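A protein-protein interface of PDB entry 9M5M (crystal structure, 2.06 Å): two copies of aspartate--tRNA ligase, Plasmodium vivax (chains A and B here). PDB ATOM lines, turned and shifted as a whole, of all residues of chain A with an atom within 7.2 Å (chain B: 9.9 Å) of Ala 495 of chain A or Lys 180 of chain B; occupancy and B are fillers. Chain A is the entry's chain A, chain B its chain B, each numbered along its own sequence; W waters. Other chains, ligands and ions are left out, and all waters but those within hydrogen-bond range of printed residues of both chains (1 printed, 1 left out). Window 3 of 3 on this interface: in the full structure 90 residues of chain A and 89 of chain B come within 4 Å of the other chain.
The guanidinium group (NH2) of Arg 95 of chain B is in hydrogen-bond range of the backbone carbonyl oxygen (O) of Asn 287 of chain A (2.9 Å). The backbone carbonyl oxygen (O) of Asn 287 of chain A lies within hydrogen-bond range of the guanidinium group (NH2) of Arg 216 of chain B, at 3.0 Å. The side-chain carboxylate of Asp 492 of chain A is in salt-bridge range of the side-chain amino group of Lys 180 of chain B (3.3 Å). The backbone carbonyl oxygen (O) of Ala 495 of chain A lies within hydrogen-bond range of the backbone NH (N) of Ala 179 of chain B, at 3.0 Å. N of Lys 180 of chain B lies within hydrogen-bond range of O of Ala 495 of chain A, 3.2 Å away. The backbone carbonyl oxygen (O) of Tyr 496 of chain A is in hydrogen-bond range of the guanidinium group (NH1) of Arg 216 of chain B, at 3.1 Å. OG of Ser 497 of chain A is in hydrogen-bond range of NE of Arg 95 of chain B, at 3.0 Å. OG of Ser 497 of chain A lies within hydrogen-bond range of O of Glu 142 of chain B (2.7 Å). The backbone NH of Ser 498 of chain A sits at hydrogen-bond distance from the side-chain hydroxyl of Ser 176 of chain B (2.9 Å).
The backbone carbonyl oxygen of Tyr 490 of chain A lies within hydrogen-bond range of the side-chain hydroxyl of Ser 493 of chain A (2.7 Å). O of Leu 141 of chain B lies within hydrogen-bond range of OG1 of Thr 178 of chain B. The guanidinium group (NH1) of Arg 216 of chain B lies within salt-bridge range of the side-chain carboxylate (OE2) of Glu 142 of chain B, 3.1 Å away. OG1 of Thr 178 of chain B lies within hydrogen-bond range of N of Ser 143 of chain B, 3.3 Å away. N of Ile 144 of chain B sits at hydrogen-bond distance from O of Ser 176 of chain B. O of Cys 212 of chain B lies within hydrogen-bond range of NE of Arg 216 of chain B (3.0 Å).
Among the printed residues, merely in contact across the chains: Asn 287 of chain A with Cys 212 of chain B (3.8 Å), Ser 493 of chain A with Cys 212 of chain B (3.6 Å), Ala 495 of chain A with Thr 178 of chain B (3.9 Å), Tyr 496 of chain A with Arg 95 of chain B (3.99 Å), Tyr 496 of chain A with Glu 142 of chain B (3.7 Å), Tyr 496 of chain A with Thr 178 of chain B (3.8 Å), Tyr 496 of chain A with Lys 180 of chain B (3.3 Å), Tyr 496 of chain A with Glu 181 of chain B (3.4 Å), Tyr 496 of chain A with Leu 182 of chain B (3.8 Å), Tyr 496 of chain A with Pro 183 of chain B (3.8 Å), Tyr 496 of chain A with Val 213 of chain B (3.7 Å), Ser 497 of chain A with Ile 144 of chain B (3.6 Å), Ser 497 of chain A with Ser 176 of chain B (3.3 Å), Ser 497 of chain A with Thr 178 of chain B (3.9 Å) and Ser 498 of chain A with Ile 144 of chain B (3.5 Å).
Asp 492 of chain A touches one residue of chain B. Printed residues of chain B within 4 Å of Ser 493 of chain A: Cys 212 (3.6 Å). Of the printed residues of chain B, Ala 495 of chain A touches Thr 178 (3.9 Å), Ala 179 (3.0 Å) and Lys 180 (3.2 Å). Lys 180 of chain B touches just these residues of chain A: Asp 492 (3.3 Å), Ala 495 (3.2 Å) and Tyr 496 (3.3 Å). Printed residues of chain A within 4 Å of Pro 183 of chain B: Tyr 496. The nearest printed residue of chain B that does not touch Tyr 496 of chain A is Asn 210 of chain B (4.4 Å).
Of the 21 printed residues of chain B, 13 touch a printed residue of chain A. Hydrophobic or aromatic side chains of chain B within 4 Å of the printed part of chain A: Ile 144, Ala 179, Leu 182, Pro 183 and Val 213. Hydrophobic or aromatic side chains of chain A that line the printed part of chain B: Tyr 496. Among the printed residues, 24 pairs touch across the chains. Among the printed residues, Asp or Glu carboxylates within 4 Å of a Lys or Arg side-chain nitrogen of the other chain: Asp 492 of chain A with Lys 180 of chain B.
No position is printed for both chains.
Water W1 lies within hydrogen-bond range of O of Ser 493 of chain A (2.6 Å), O of Ser 497 of chain A (2.7 Å), N of Tyr 496 of chain A (2.8 Å) and NH2 of Arg 216 of chain B (2.8 Å).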
ATOM      1  N   ASN A 287      -6.044 -20.030  -9.214  1.00  0.00           N
ATOM      2  CA  ASN A 287      -5.125 -20.668  -8.284  1.00  0.00           C
ATOM      3  C   ASN A 287      -5.030 -19.916  -6.968  1.00  0.00           C
ATOM      4  O   ASN A 287      -4.518 -20.480  -6.002  1.00  0.00           O
ATOM      5  CB  ASN A 287      -3.732 -20.795  -8.898  1.00  0.00           C
ATOM      6  CG  ASN A 287      -3.665 -21.851  -9.987  1.00  0.00           C
ATOM      7  OD1 ASN A 287      -4.405 -22.838  -9.968  1.00  0.00           O
ATOM      8  ND2 ASN A 287      -2.753 -21.658 -10.938  1.00  0.00           N
ATOM      9  N   VAL A 470       1.040 -29.222 -11.405  1.00  0.00           N
ATOM     10  CA  VAL A 470       2.197 -28.418 -11.789  1.00  0.00           C
ATOM     11  C   VAL A 470       3.207 -29.255 -12.564  1.00  0.00           C
ATOM     12  O   VAL A 470       3.857 -28.755 -13.493  1.00  0.00           O
ATOM     13  CB  VAL A 470       2.815 -27.762 -10.538  1.00  0.00           C
ATOM     14  CG1 VAL A 470       3.269 -28.816  -9.545  1.00  0.00           C
ATOM     15  CG2 VAL A 470       3.965 -26.864 -10.922  1.00  0.00           C
ATOM     16  N   TYR A 490       3.725 -17.869 -13.839  1.00  0.00           N
ATOM     17  CA  TYR A 490       2.518 -18.632 -14.100  1.00  0.00           C
ATOM     18  C   TYR A 490       2.660 -20.044 -13.568  1.00  0.00           C
ATOM     19  O   TYR A 490       1.798 -20.526 -12.823  1.00  0.00           O
ATOM     20  CB  TYR A 490       2.243 -18.625 -15.600  1.00  0.00           C
ATOM     21  CG  TYR A 490       1.197 -19.592 -16.096  1.00  0.00           C
ATOM     22  CD1 TYR A 490      -0.156 -19.319 -15.943  1.00  0.00           C
ATOM     23  CD2 TYR A 490       1.564 -20.764 -16.753  1.00  0.00           C
ATOM     24  CE1 TYR A 490      -1.121 -20.181 -16.431  1.00  0.00           C
ATOM     25  CE2 TYR A 490       0.601 -21.643 -17.242  1.00  0.00           C
ATOM     26  CZ  TYR A 490      -0.736 -21.338 -17.083  1.00  0.00           C
ATOM     27  OH  TYR A 490      -1.693 -22.193 -17.571  1.00  0.00           O
ATOM     28  N   ILE A 491       3.769 -20.710 -13.902  1.00  0.00           N
ATOM     29  CA  ILE A 491       3.963 -22.074 -13.418  1.00  0.00           C
ATOM     30  C   ILE A 491       3.961 -22.076 -11.899  1.00  0.00           C
ATOM     31  O   ILE A 491       3.404 -22.978 -11.257  1.00  0.00           O
ATOM     32  CB  ILE A 491       5.270 -22.665 -13.976  1.00  0.00           C
ATOM     33  CG1 ILE A 491       5.222 -22.753 -15.504  1.00  0.00           C
ATOM     34  CG2 ILE A 491       5.596 -24.022 -13.314  1.00  0.00           C
ATOM     35  CD1 ILE A 491       6.618 -22.858 -16.119  1.00  0.00           C
ATOM     36  N   ASP A 492       4.535 -21.033 -11.291  1.00  0.00           N
ATOM     37  CA  ASP A 492       4.687 -21.121  -9.850  1.00  0.00           C
ATOM     38  C   ASP A 492       3.344 -20.955  -9.163  1.00  0.00           C
ATOM     39  O   ASP A 492       3.182 -21.415  -8.023  1.00  0.00           O
ATOM     40  CB  ASP A 492       5.716 -20.099  -9.355  1.00  0.00           C
ATOM     41  CG  ASP A 492       5.985 -20.217  -7.873  1.00  0.00           C
ATOM     42  OD1 ASP A 492       5.642 -19.266  -7.132  1.00  0.00           O
ATOM     43  OD2 ASP A 492       6.515 -21.261  -7.441  1.00  0.00           O
ATOM     44  N   SER A 493       2.353 -20.391  -9.869  1.00  0.00           N
ATOM     45  CA  SER A 493       1.036 -20.289  -9.254  1.00  0.00           C
ATOM     46  C   SER A 493       0.349 -21.645  -9.103  1.00  0.00           C
ATOM     47  O   SER A 493      -0.662 -21.727  -8.397  1.00  0.00           O
ATOM     48  CB  SER A 493       0.147 -19.340 -10.053  1.00  0.00           C
ATOM     49  OG  SER A 493      -0.292 -19.966 -11.246  1.00  0.00           O
ATOM     50  N   PHE A 494       0.868 -22.709  -9.728  1.00  0.00           N
ATOM     51  CA  PHE A 494       0.287 -24.039  -9.555  1.00  0.00           C
ATOM     52  C   PHE A 494       1.000 -24.876  -8.494  1.00  0.00           C
ATOM     53  O   PHE A 494       0.569 -26.002  -8.227  1.00  0.00           O
ATOM     54  CB  PHE A 494       0.305 -24.823 -10.880  1.00  0.00           C
ATOM     55  CG  PHE A 494      -0.470 -24.176 -11.988  1.00  0.00           C
ATOM     56  CD1 PHE A 494      -1.738 -24.628 -12.319  1.00  0.00           C
ATOM     57  CD2 PHE A 494       0.081 -23.136 -12.715  1.00  0.00           C
ATOM     58  CE1 PHE A 494      -2.459 -24.027 -13.350  1.00  0.00           C
ATOM     59  CE2 PHE A 494      -0.626 -22.534 -13.741  1.00  0.00           C
ATOM     60  CZ  PHE A 494      -1.896 -22.981 -14.066  1.00  0.00           C
ATOM     61  N   ALA A 495       2.075 -24.369  -7.894  1.00  0.00           N
ATOM     62  CA  ALA A 495       2.917 -25.178  -7.021  1.00  0.00           C
ATOM     63  C   ALA A 495       2.426 -25.225  -5.574  1.00  0.00           C
ATOM     64  O   ALA A 495       3.055 -25.901  -4.747  1.00  0.00           O
ATOM     65  CB  ALA A 495       4.355 -24.657  -7.062  1.00  0.00           C
ATOM     66  N   TYR A 496       1.336 -24.529  -5.237  1.00  0.00           N
ATOM     67  CA  TYR A 496       0.814 -24.598  -3.874  1.00  0.00           C
ATOM     68  C   TYR A 496      -0.644 -25.022  -3.934  1.00  0.00           C
ATOM     69  O   TYR A 496      -1.511 -24.403  -3.304  1.00  0.00           O
ATOM     70  CB  TYR A 496       0.981 -23.262  -3.142  1.00  0.00           C
ATOM     71  CG  TYR A 496       2.282 -22.566  -3.476  1.00  0.00           C
ATOM     72  CD1 TYR A 496       3.465 -22.906  -2.830  1.00  0.00           C
ATOM     73  CD2 TYR A 496       2.335 -21.585  -4.466  1.00  0.00           C
ATOM     74  CE1 TYR A 496       4.658 -22.278  -3.146  1.00  0.00           C
ATOM     75  CE2 TYR A 496       3.526 -20.956  -4.786  1.00  0.00           C
ATOM     76  CZ  TYR A 496       4.680 -21.307  -4.120  1.00  0.00           C
ATOM     77  OH  TYR A 496       5.858 -20.676  -4.439  1.00  0.00           O
ATOM     78  N   SER A 497      -0.889 -26.085  -4.711  1.00  0.00           N
ATOM     79  CA  SER A 497      -2.180 -26.701  -4.993  1.00  0.00           C
ATOM     80  C   SER A 497      -2.908 -25.918  -6.073  1.00  0.00           C
ATOM     81  O   SER A 497      -2.659 -24.725  -6.275  1.00  0.00           O
ATOM     82  CB  SER A 497      -3.053 -26.828  -3.739  1.00  0.00           C
ATOM     83  OG  SER A 497      -3.652 -25.589  -3.396  1.00  0.00           O
ATOM     84  N   SER A 498      -3.789 -26.599  -6.791  1.00  0.00           N
ATOM     85  CA  SER A 498      -4.554 -25.973  -7.855  1.00  0.00           C
ATOM     86  C   SER A 498      -5.907 -26.659  -7.930  1.00  0.00           C
ATOM     87  O   SER A 498      -5.979 -27.894  -7.950  1.00  0.00           O
ATOM     88  CB  SER A 498      -3.823 -26.072  -9.198  1.00  0.00           C
ATOM     89  OG  SER A 498      -4.621 -25.557 -10.251  1.00  0.00           O
ATOM     90  N   ARG B  95      -9.211 -25.706   1.148  1.00  0.00           N
ATOM     91  CA  ARG B  95      -7.767 -25.691   1.353  1.00  0.00           C
ATOM     92  C   ARG B  95      -7.448 -25.838   2.834  1.00  0.00           C
ATOM     93  O   ARG B  95      -8.159 -25.313   3.695  1.00  0.00           O
ATOM     94  CB  ARG B  95      -7.129 -24.409   0.806  1.00  0.00           C
ATOM     95  CG  ARG B  95      -6.747 -24.520  -0.661  1.00  0.00           C
ATOM     96  CD  ARG B  95      -6.150 -23.254  -1.251  1.00  0.00           C
ATOM     97  NE  ARG B  95      -5.646 -23.530  -2.594  1.00  0.00           N
ATOM     98  CZ  ARG B  95      -5.462 -22.622  -3.544  1.00  0.00           C
ATOM     99  NH1 ARG B  95      -5.752 -21.346  -3.350  1.00  0.00           N
ATOM    100  NH2 ARG B  95      -4.969 -23.005  -4.716  1.00  0.00           N
ATOM    101  N   PRO B 140       0.679 -31.187   3.563  1.00  0.00           N
ATOM    102  CA  PRO B 140       1.186 -29.808   3.568  1.00  0.00           C
ATOM    103  C   PRO B 140       0.051 -28.795   3.607  1.00  0.00           C
ATOM    104  O   PRO B 140      -1.050 -29.040   3.108  1.00  0.00           O
ATOM    105  CB  PRO B 140       1.954 -29.690   2.243  1.00  0.00           C
ATOM    106  CG  PRO B 140       1.880 -31.013   1.584  1.00  0.00           C
ATOM    107  CD  PRO B 140       0.828 -31.836   2.253  1.00  0.00           C
ATOM    108  N   LEU B 141       0.336 -27.637   4.200  1.00  0.00           N
ATOM    109  CA  LEU B 141      -0.643 -26.564   4.192  1.00  0.00           C
ATOM    110  C   LEU B 141      -0.884 -26.090   2.760  1.00  0.00           C
ATOM    111  O   LEU B 141       0.020 -26.109   1.919  1.00  0.00           O
ATOM    112  CB  LEU B 141      -0.175 -25.401   5.069  1.00  0.00           C
ATOM    113  CG  LEU B 141      -0.135 -25.665   6.581  1.00  0.00           C
ATOM    114  CD1 LEU B 141       0.272 -24.401   7.329  1.00  0.00           C
ATOM    115  CD2 LEU B 141      -1.486 -26.154   7.075  1.00  0.00           C
ATOM    116  N   GLU B 142      -2.125 -25.673   2.496  1.00  0.00           N
ATOM    117  CA  GLU B 142      -2.699 -25.221   1.222  1.00  0.00           C
ATOM    118  C   GLU B 142      -3.169 -26.381   0.347  1.00  0.00           C
ATOM    119  O   GLU B 142      -3.718 -26.118  -0.721  1.00  0.00           O
ATOM    120  CB  GLU B 142      -1.755 -24.335   0.391  1.00  0.00           C
ATOM    121  CG  GLU B 142      -1.499 -22.971   1.003  1.00  0.00           C
ATOM    122  CD  GLU B 142      -2.793 -22.252   1.362  1.00  0.00           C
ATOM    123  OE1 GLU B 142      -3.137 -22.214   2.562  1.00  0.00           O
ATOM    124  OE2 GLU B 142      -3.479 -21.751   0.440  1.00  0.00           O
ATOM    125  N   SER B 143      -2.991 -27.636   0.756  1.00  0.00           N
ATOM    126  CA  SER B 143      -3.491 -28.752  -0.041  1.00  0.00           C
ATOM    127  C   SER B 143      -5.014 -28.706  -0.131  1.00  0.00           C
ATOM    128  O   SER B 143      -5.701 -28.329   0.819  1.00  0.00           O
ATOM    129  CB  SER B 143      -3.055 -30.090   0.568  1.00  0.00           C
ATOM    130  OG  SER B 143      -1.645 -30.184   0.708  1.00  0.00           O
ATOM    131  N   ILE B 144      -5.548 -29.103  -1.279  1.00  0.00           N
ATOM    132  CA  ILE B 144      -6.989 -29.097  -1.498  1.00  0.00           C
ATOM    133  C   ILE B 144      -7.527 -30.492  -1.216  1.00  0.00           C
ATOM    134  O   ILE B 144      -7.074 -31.473  -1.820  1.00  0.00           O
ATOM    135  CB  ILE B 144      -7.345 -28.643  -2.921  1.00  0.00           C
ATOM    136  CG1 ILE B 144      -6.856 -27.216  -3.155  1.00  0.00           C
ATOM    137  CG2 ILE B 144      -8.839 -28.734  -3.126  1.00  0.00           C
ATOM    138  CD1 ILE B 144      -6.907 -26.783  -4.612  1.00  0.00           C
ATOM    139  N   SER B 176      -5.372 -32.255  -4.556  1.00  0.00           N
ATOM    140  CA  SER B 176      -4.247 -31.454  -5.024  1.00  0.00           C
ATOM    141  C   SER B 176      -3.337 -31.185  -3.837  1.00  0.00           C
ATOM    142  O   SER B 176      -3.719 -30.494  -2.887  1.00  0.00           O
ATOM    143  CB  SER B 176      -4.708 -30.148  -5.664  1.00  0.00           C
ATOM    144  OG  SER B 176      -3.601 -29.416  -6.153  1.00  0.00           O
ATOM    145  N   LYS B 177      -2.135 -31.734  -3.894  1.00  0.00           N
ATOM    146  CA  LYS B 177      -1.172 -31.623  -2.816  1.00  0.00           C
ATOM    147  C   LYS B 177      -0.212 -30.482  -3.119  1.00  0.00           C
ATOM    148  O   LYS B 177       0.347 -30.415  -4.219  1.00  0.00           O
ATOM    149  CB  LYS B 177      -0.415 -32.939  -2.655  1.00  0.00           C
ATOM    150  CG  LYS B 177       0.748 -32.896  -1.684  1.00  0.00           C
ATOM    151  CD  LYS B 177       1.515 -34.209  -1.714  1.00  0.00           C
ATOM    152  CE  LYS B 177       3.015 -33.966  -1.775  1.00  0.00           C
ATOM    153  NZ  LYS B 177       3.470 -33.073  -0.667  1.00  0.00           N
ATOM    154  N   THR B 178      -0.042 -29.576  -2.155  1.00  0.00           N
ATOM    155  CA  THR B 178       0.990 -28.553  -2.276  1.00  0.00           C
ATOM    156  C   THR B 178       2.316 -29.217  -2.629  1.00  0.00           C
ATOM    157  O   THR B 178       2.730 -30.173  -1.977  1.00  0.00           O
ATOM    158  CB  THR B 178       1.117 -27.772  -0.962  1.00  0.00           C
ATOM    159  OG1 THR B 178      -0.111 -27.087  -0.680  1.00  0.00           O
ATOM    160  CG2 THR B 178       2.237 -26.754  -1.057  1.00  0.00           C
ATOM    161  N   ALA B 179       2.962 -28.736  -3.686  1.00  0.00           N
ATOM    162  CA  ALA B 179       4.186 -29.373  -4.161  1.00  0.00           C
ATOM    163  C   ALA B 179       5.451 -28.732  -3.607  1.00  0.00           C
ATOM    164  O   ALA B 179       6.506 -29.372  -3.599  1.00  0.00           O
ATOM    165  CB  ALA B 179       4.242 -29.337  -5.694  1.00  0.00           C
ATOM    166  N   LYS B 180       5.366 -27.495  -3.143  1.00  0.00           N
ATOM    167  CA  LYS B 180       6.531 -26.679  -2.852  1.00  0.00           C
ATOM    168  C   LYS B 180       6.286 -25.903  -1.564  1.00  0.00           C
ATOM    169  O   LYS B 180       5.151 -25.528  -1.261  1.00  0.00           O
ATOM    170  CB  LYS B 180       6.799 -25.721  -4.027  1.00  0.00           C
ATOM    171  CG  LYS B 180       7.884 -24.708  -3.784  1.00  0.00           C
ATOM    172  CD  LYS B 180       7.641 -23.466  -4.614  1.00  0.00           C
ATOM    173  CE  LYS B 180       8.362 -23.536  -5.928  1.00  0.00           C
ATOM    174  NZ  LYS B 180       9.309 -22.407  -6.064  1.00  0.00           N
ATOM    175  N   GLU B 181       7.356 -25.672  -0.807  1.00  0.00           N
ATOM    176  CA  GLU B 181       7.260 -24.851   0.393  1.00  0.00           C
ATOM    177  C   GLU B 181       6.793 -23.439   0.039  1.00  0.00           C
ATOM    178  O   GLU B 181       7.218 -22.851  -0.960  1.00  0.00           O
ATOM    179  CB  GLU B 181       8.612 -24.799   1.102  1.00  0.00           C
ATOM    180  CG  GLU B 181       8.541 -24.375   2.555  1.00  0.00           C
ATOM    181  CD  GLU B 181       8.076 -25.496   3.460  1.00  0.00           C
ATOM    182  OE1 GLU B 181       8.355 -26.671   3.138  1.00  0.00           O
ATOM    183  OE2 GLU B 181       7.431 -25.206   4.491  1.00  0.00           O
ATOM    184  N   LEU B 182       5.905 -22.894   0.862  1.00  0.00           N
ATOM    185  CA  LEU B 182       5.355 -21.583   0.568  1.00  0.00           C
ATOM    186  C   LEU B 182       6.423 -20.499   0.729  1.00  0.00           C
ATOM    187  O   LEU B 182       7.341 -20.637   1.533  1.00  0.00           O
ATOM    188  CB  LEU B 182       4.160 -21.293   1.474  1.00  0.00           C
ATOM    189  CG  LEU B 182       2.819 -21.677   0.838  1.00  0.00           C
ATOM    190  CD1 LEU B 182       2.392 -23.079   1.247  1.00  0.00           C
ATOM    191  CD2 LEU B 182       1.755 -20.654   1.184  1.00  0.00           C
ATOM    192  N   PRO B 183       6.326 -19.412  -0.034  1.00  0.00           N
ATOM    193  CA  PRO B 183       7.312 -18.330   0.120  1.00  0.00           C
ATOM    194  C   PRO B 183       7.219 -17.639   1.467  1.00  0.00           C
ATOM    195  O   PRO B 183       8.198 -17.035   1.921  1.00  0.00           O
ATOM    196  CB  PRO B 183       6.963 -17.379  -1.031  1.00  0.00           C
ATOM    197  CG  PRO B 183       5.513 -17.646  -1.301  1.00  0.00           C
ATOM    198  CD  PRO B 183       5.319 -19.105  -1.062  1.00  0.00           C
ATOM    199  N   PHE B 184       6.055 -17.701   2.103  1.00  0.00           N
ATOM    200  CA  PHE B 184       5.840 -17.233   3.463  1.00  0.00           C
ATOM    201  C   PHE B 184       4.586 -17.934   3.962  1.00  0.00           C
ATOM    202  O   PHE B 184       3.838 -18.526   3.182  1.00  0.00           O
ATOM    203  CB  PHE B 184       5.694 -15.709   3.523  1.00  0.00           C
ATOM    204  CG  PHE B 184       4.808 -15.135   2.446  1.00  0.00           C
ATOM    205  CD1 PHE B 184       5.360 -14.447   1.376  1.00  0.00           C
ATOM    206  CD2 PHE B 184       3.430 -15.285   2.504  1.00  0.00           C
ATOM    207  CE1 PHE B 184       4.569 -13.916   0.389  1.00  0.00           C
ATOM    208  CE2 PHE B 184       2.618 -14.756   1.510  1.00  0.00           C
ATOM    209  CZ  PHE B 184       3.188 -14.070   0.453  1.00  0.00           C
ATOM    210  N   LEU B 185       4.360 -17.862   5.268  1.00  0.00           N
ATOM    211  CA  LEU B 185       3.196 -18.501   5.868  1.00  0.00           C
ATOM    212  C   LEU B 185       1.982 -17.583   5.797  1.00  0.00           C
ATOM    213  O   LEU B 185       2.085 -16.382   6.059  1.00  0.00           O
ATOM    214  CB  LEU B 185       3.487 -18.867   7.320  1.00  0.00           C
ATOM    215  CG  LEU B 185       4.719 -19.748   7.519  1.00  0.00           C
ATOM    216  CD1 LEU B 185       5.247 -19.651   8.960  1.00  0.00           C
ATOM    217  CD2 LEU B 185       4.380 -21.184   7.174  1.00  0.00           C
ATOM    218  N   ASN B 209       5.946 -10.351  -5.511  1.00  0.00           N
ATOM    219  CA  ASN B 209       6.669 -11.347  -6.275  1.00  0.00           C
ATOM    220  C   ASN B 209       6.002 -12.686  -6.122  1.00  0.00           C
ATOM    221  O   ASN B 209       6.265 -13.586  -6.872  1.00  0.00           O
ATOM    222  CB  ASN B 209       8.121 -11.465  -5.851  1.00  0.00           C
ATOM    223  CG  ASN B 209       8.915 -10.236  -6.145  1.00  0.00           C
ATOM    224  OD1 ASN B 209       8.508  -9.393  -6.901  1.00  0.00           O
ATOM    225  ND2 ASN B 209      10.059 -10.130  -5.533  1.00  0.00           N
ATOM    226  N   ASN B 210       5.141 -12.823  -5.134  1.00  0.00           N
ATOM    227  CA  ASN B 210       4.437 -14.055  -4.917  1.00  0.00           C
ATOM    228  C   ASN B 210       2.958 -13.790  -4.810  1.00  0.00           C
ATOM    229  O   ASN B 210       2.275 -14.379  -4.013  1.00  0.00           O
ATOM    230  CB  ASN B 210       4.939 -14.713  -3.653  1.00  0.00           C
ATOM    231  CG  ASN B 210       6.341 -15.256  -3.796  1.00  0.00           C
ATOM    232  OD1 ASN B 210       6.533 -16.348  -4.260  1.00  0.00           O
ATOM    233  ND2 ASN B 210       7.307 -14.478  -3.418  1.00  0.00           N
ATOM    234  N   CYS B 212       0.309 -14.740  -6.115  1.00  0.00           N
ATOM    235  CA  CYS B 212      -0.702 -15.791  -6.082  1.00  0.00           C
ATOM    236  C   CYS B 212      -0.865 -16.405  -4.696  1.00  0.00           C
ATOM    237  O   CYS B 212      -1.921 -16.986  -4.407  1.00  0.00           O
ATOM    238  CB  CYS B 212      -0.363 -16.894  -7.079  1.00  0.00           C
ATOM    239  SG  CYS B 212      -1.613 -18.214  -7.091  1.00  0.00           S
ATOM    240  N   VAL B 213       0.159 -16.317  -3.846  1.00  0.00           N
ATOM    241  CA  VAL B 213      -0.006 -16.656  -2.436  1.00  0.00           C
ATOM    242  C   VAL B 213      -0.539 -15.462  -1.652  1.00  0.00           C
ATOM    243  O   VAL B 213      -1.399 -15.613  -0.778  1.00  0.00           O
ATOM    244  CB  VAL B 213       1.339 -17.151  -1.863  1.00  0.00           C
ATOM    245  CG1 VAL B 213       1.214 -17.462  -0.379  1.00  0.00           C
ATOM    246  CG2 VAL B 213       1.822 -18.372  -2.634  1.00  0.00           C
ATOM    247  N   ARG B 216      -4.337 -14.860  -1.228  1.00  0.00           N
ATOM    248  CA  ARG B 216      -5.119 -15.767  -0.396  1.00  0.00           C
ATOM    249  C   ARG B 216      -5.356 -15.246   1.017  1.00  0.00           C
ATOM    250  O   ARG B 216      -6.134 -15.865   1.758  1.00  0.00           O
ATOM    251  CB  ARG B 216      -4.438 -17.143  -0.310  1.00  0.00           C
ATOM    252  CG  ARG B 216      -4.239 -17.802  -1.671  1.00  0.00           C
ATOM    253  CD  ARG B 216      -3.322 -19.019  -1.613  1.00  0.00           C
ATOM    254  NE  ARG B 216      -2.855 -19.379  -2.954  1.00  0.00           N
ATOM    255  CZ  ARG B 216      -2.320 -20.550  -3.274  1.00  0.00           C
ATOM    256  NH1 ARG B 216      -2.204 -21.526  -2.382  1.00  0.00           N
ATOM    257  NH2 ARG B 216      -1.893 -20.750  -4.516  1.00  0.00           N
HETATM  258  O   HOH W   1      -0.758 -22.837  -6.047  1.00  0.00           O
